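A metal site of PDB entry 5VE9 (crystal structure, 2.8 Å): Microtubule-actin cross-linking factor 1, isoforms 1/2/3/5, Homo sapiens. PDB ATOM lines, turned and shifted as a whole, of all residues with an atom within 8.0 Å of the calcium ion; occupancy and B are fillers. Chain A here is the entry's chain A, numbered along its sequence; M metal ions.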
ATOM      1  N   PHE A  33       8.202  30.719 -21.914  1.00  0.00           N
ATOM      2  CA  PHE A  33       7.649  29.702 -22.810  1.00  0.00           C
ATOM      3  C   PHE A  33       8.644  28.566 -23.055  1.00  0.00           C
ATOM      4  O   PHE A  33       8.295  27.388 -22.933  1.00  0.00           O
ATOM      5  CB  PHE A  33       7.246  30.307 -24.158  1.00  0.00           C
ATOM      6  CG  PHE A  33       6.492  29.362 -25.041  1.00  0.00           C
ATOM      7  CD1 PHE A  33       5.111  29.397 -25.112  1.00  0.00           C
ATOM      8  CD2 PHE A  33       7.163  28.416 -25.808  1.00  0.00           C
ATOM      9  CE1 PHE A  33       4.405  28.522 -25.927  1.00  0.00           C
ATOM     10  CE2 PHE A  33       6.470  27.536 -26.619  1.00  0.00           C
ATOM     11  CZ  PHE A  33       5.092  27.587 -26.684  1.00  0.00           C
ATOM     12  N   ILE A  36       9.011  26.370 -20.037  1.00  0.00           N
ATOM     13  CA  ILE A  36       7.864  25.470 -19.865  1.00  0.00           C
ATOM     14  C   ILE A  36       7.842  24.410 -20.957  1.00  0.00           C
ATOM     15  O   ILE A  36       7.403  23.282 -20.733  1.00  0.00           O
ATOM     16  CB  ILE A  36       6.524  26.246 -19.882  1.00  0.00           C
ATOM     17  CG1 ILE A  36       6.467  27.244 -18.717  1.00  0.00           C
ATOM     18  CG2 ILE A  36       5.351  25.286 -19.806  1.00  0.00           C
ATOM     19  CD1 ILE A  36       6.549  26.608 -17.345  1.00  0.00           C
ATOM     20  N   ASP A  37       8.293  24.780 -22.160  1.00  0.00           N
ATOM     21  CA  ASP A  37       8.371  23.845 -23.274  1.00  0.00           C
ATOM     22  C   ASP A  37       9.613  22.965 -23.155  1.00  0.00           C
ATOM     23  O   ASP A  37      10.658  23.256 -23.745  1.00  0.00           O
ATOM     24  CB  ASP A  37       8.364  24.596 -24.606  1.00  0.00           C
ATOM     25  CG  ASP A  37       8.416  23.665 -25.803  1.00  0.00           C
ATOM     26  OD1 ASP A  37       7.992  22.506 -25.672  1.00  0.00           O
ATOM     27  OD2 ASP A  37       8.901  24.099 -26.876  1.00  0.00           O
ATOM     28  N   LYS A  38       9.504  21.890 -22.380  1.00  0.00           N
ATOM     29  CA  LYS A  38      10.645  21.021 -22.098  1.00  0.00           C
ATOM     30  C   LYS A  38      11.021  20.127 -23.276  1.00  0.00           C
ATOM     31  O   LYS A  38      12.193  19.854 -23.500  1.00  0.00           O
ATOM     32  CB  LYS A  38      10.348  20.163 -20.865  1.00  0.00           C
ATOM     33  CG  LYS A  38       9.975  20.963 -19.637  1.00  0.00           C
ATOM     34  CD  LYS A  38      10.077  20.139 -18.356  1.00  0.00           C
ATOM     35  CE  LYS A  38       9.679  20.949 -17.137  1.00  0.00           C
ATOM     36  NZ  LYS A  38      10.449  22.232 -17.023  1.00  0.00           N
ATOM     37  N   ASP A  39      10.018  19.663 -24.018  1.00  0.00           N
ATOM     38  CA  ASP A  39      10.261  18.813 -25.179  1.00  0.00           C
ATOM     39  C   ASP A  39      10.797  19.618 -26.357  1.00  0.00           C
ATOM     40  O   ASP A  39      11.210  19.059 -27.366  1.00  0.00           O
ATOM     41  CB  ASP A  39       9.000  18.051 -25.590  1.00  0.00           C
ATOM     42  CG  ASP A  39       7.765  18.937 -25.612  1.00  0.00           C
ATOM     43  OD1 ASP A  39       7.703  19.900 -24.823  1.00  0.00           O
ATOM     44  OD2 ASP A  39       6.853  18.656 -26.426  1.00  0.00           O
ATOM     45  N   GLN A  40      10.790  20.947 -26.217  1.00  0.00           N
ATOM     46  CA  GLN A  40      11.406  21.841 -27.197  1.00  0.00           C
ATOM     47  C   GLN A  40      10.871  21.646 -28.626  1.00  0.00           C
ATOM     48  O   GLN A  40      11.647  21.580 -29.578  1.00  0.00           O
ATOM     49  CB  GLN A  40      12.928  21.637 -27.202  1.00  0.00           C
ATOM     50  CG  GLN A  40      13.600  21.920 -25.871  1.00  0.00           C
ATOM     51  CD  GLN A  40      13.509  23.386 -25.470  1.00  0.00           C
ATOM     52  OE1 GLN A  40      13.524  24.277 -26.323  1.00  0.00           O
ATOM     53  NE2 GLN A  40      13.414  23.637 -24.174  1.00  0.00           N
ATOM     54  N   ASP A  41       9.546  21.576 -28.760  1.00  0.00           N
ATOM     55  CA  ASP A  41       8.917  21.412 -30.072  1.00  0.00           C
ATOM     56  C   ASP A  41       7.973  22.564 -30.397  1.00  0.00           C
ATOM     57  O   ASP A  41       7.278  22.535 -31.411  1.00  0.00           O
ATOM     58  CB  ASP A  41       8.163  20.079 -30.125  1.00  0.00           C
ATOM     59  CG  ASP A  41       6.934  20.061 -29.232  1.00  0.00           C
ATOM     60  OD1 ASP A  41       6.850  20.893 -28.314  1.00  0.00           O
ATOM     61  OD2 ASP A  41       6.050  19.203 -29.465  1.00  0.00           O
ATOM     62  N   GLY A  42       7.937  23.569 -29.528  1.00  0.00           N
ATOM     63  CA  GLY A  42       7.169  24.776 -29.781  1.00  0.00           C
ATOM     64  C   GLY A  42       5.714  24.699 -29.357  1.00  0.00           C
ATOM     65  O   GLY A  42       4.914  25.520 -29.796  1.00  0.00           O
ATOM     66  N   LYS A  43       5.377  23.741 -28.513  1.00  0.00           N
ATOM     67  CA  LYS A  43       4.009  23.596 -28.004  1.00  0.00           C
ATOM     68  C   LYS A  43       4.003  23.404 -26.493  1.00  0.00           C
ATOM     69  O   LYS A  43       4.953  22.871 -25.917  1.00  0.00           O
ATOM     70  CB  LYS A  43       3.307  22.410 -28.675  1.00  0.00           C
ATOM     71  CG  LYS A  43       3.234  22.486 -30.194  1.00  0.00           C
ATOM     72  CD  LYS A  43       2.978  21.111 -30.816  1.00  0.00           C
ATOM     73  CE  LYS A  43       1.559  20.615 -30.561  1.00  0.00           C
ATOM     74  NZ  LYS A  43       1.412  19.158 -30.864  1.00  0.00           N
ATOM     75  N   ILE A  44       2.931  23.857 -25.856  1.00  0.00           N
ATOM     76  CA  ILE A  44       2.669  23.552 -24.453  1.00  0.00           C
ATOM     77  C   ILE A  44       1.170  23.371 -24.278  1.00  0.00           C
ATOM     78  O   ILE A  44       0.373  24.127 -24.858  1.00  0.00           O
ATOM     79  CB  ILE A  44       3.189  24.650 -23.492  1.00  0.00           C
ATOM     80  CG1 ILE A  44       2.604  26.017 -23.852  1.00  0.00           C
ATOM     81  CG2 ILE A  44       4.724  24.692 -23.532  1.00  0.00           C
ATOM     82  CD1 ILE A  44       3.052  27.137 -22.936  1.00  0.00           C
ATOM     83  N   THR A  45       0.764  22.366 -23.512  1.00  0.00           N
ATOM     84  CA  THR A  45      -0.644  22.132 -23.245  1.00  0.00           C
ATOM     85  C   THR A  45      -1.240  23.306 -22.502  1.00  0.00           C
ATOM     86  O   THR A  45      -0.517  24.066 -21.853  1.00  0.00           O
ATOM     87  CB  THR A  45      -0.872  20.844 -22.417  1.00  0.00           C
ATOM     88  OG1 THR A  45      -0.233  20.974 -21.146  1.00  0.00           O
ATOM     89  CG2 THR A  45      -0.334  19.627 -23.151  1.00  0.00           C
ATOM     90  N   GLU A  48      -0.116  22.811 -18.936  1.00  0.00           N
ATOM     91  CA  GLU A  48       1.286  23.168 -18.705  1.00  0.00           C
ATOM     92  C   GLU A  48       1.433  24.684 -18.634  1.00  0.00           C
ATOM     93  O   GLU A  48       2.201  25.212 -17.831  1.00  0.00           O
ATOM     94  CB  GLU A  48       2.196  22.613 -19.814  1.00  0.00           C
ATOM     95  CG  GLU A  48       2.509  21.126 -19.681  1.00  0.00           C
ATOM     96  CD  GLU A  48       3.360  20.612 -20.827  1.00  0.00           C
ATOM     97  OE1 GLU A  48       4.240  19.763 -20.574  1.00  0.00           O
ATOM     98  OE2 GLU A  48       3.139  21.035 -21.980  1.00  0.00           O
ATOM     99  N   TYR A  79      -3.427  22.508 -27.572  1.00  0.00           N
ATOM    100  CA  TYR A  79      -2.047  22.975 -27.389  1.00  0.00           C
ATOM    101  C   TYR A  79      -1.890  24.449 -27.699  1.00  0.00           C
ATOM    102  O   TYR A  79      -2.439  24.940 -28.686  1.00  0.00           O
ATOM    103  CB  TYR A  79      -1.102  22.192 -28.295  1.00  0.00           C
ATOM    104  CG  TYR A  79      -0.813  20.791 -27.828  1.00  0.00           C
ATOM    105  CD1 TYR A  79       0.155  20.553 -26.872  1.00  0.00           C
ATOM    106  CD2 TYR A  79      -1.502  19.710 -28.366  1.00  0.00           C
ATOM    107  CE1 TYR A  79       0.430  19.267 -26.452  1.00  0.00           C
ATOM    108  CE2 TYR A  79      -1.228  18.429 -27.959  1.00  0.00           C
ATOM    109  CZ  TYR A  79      -0.263  18.218 -26.990  1.00  0.00           C
ATOM    110  OH  TYR A  79       0.003  16.927 -26.572  1.00  0.00           O
ATOM    111  N   ILE A  80      -1.117  25.151 -26.870  1.00  0.00           N
ATOM    112  CA  ILE A  80      -0.726  26.526 -27.178  1.00  0.00           C
ATOM    113  C   ILE A  80       0.643  26.517 -27.846  1.00  0.00           C
ATOM    114  O   ILE A  80       1.655  26.237 -27.187  1.00  0.00           O
ATOM    115  CB  ILE A  80      -0.709  27.408 -25.917  1.00  0.00           C
ATOM    116  CG1 ILE A  80      -2.029  27.264 -25.161  1.00  0.00           C
ATOM    117  CG2 ILE A  80      -0.447  28.864 -26.292  1.00  0.00           C
ATOM    118  CD1 ILE A  80      -2.091  28.045 -23.870  1.00  0.00           C
HETATM  119 CA    CA M   1       5.850  20.775 -26.102  1.00  0.00          CA
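N of Gly 42 is in hydrogen-bond range of OD2 of Asp 37.
NE2 of Gln 40 is in hydrogen-bond range of O of Asp 37, 2.8 Å away.
Within 4 Å of the calcium ion: Asp 37, Asp 39, Asp 41 and Lys 43.
The calcium ion is bound by the backbone carbonyl oxygen (O) of Lys 43 (2.3 Å), the side-chain carboxylate (OD2) of Asp 39 (2.4 Å), the side-chain carboxylate (OD1) of Asp 39 (2.4 Å), the side-chain carboxylate (OD1) of Asp 41 (2.4 Å) and the side-chain carboxylate (OD1) of Asp 37 (2.8 Å).
The calcium ion has five donor atoms within binding distance.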
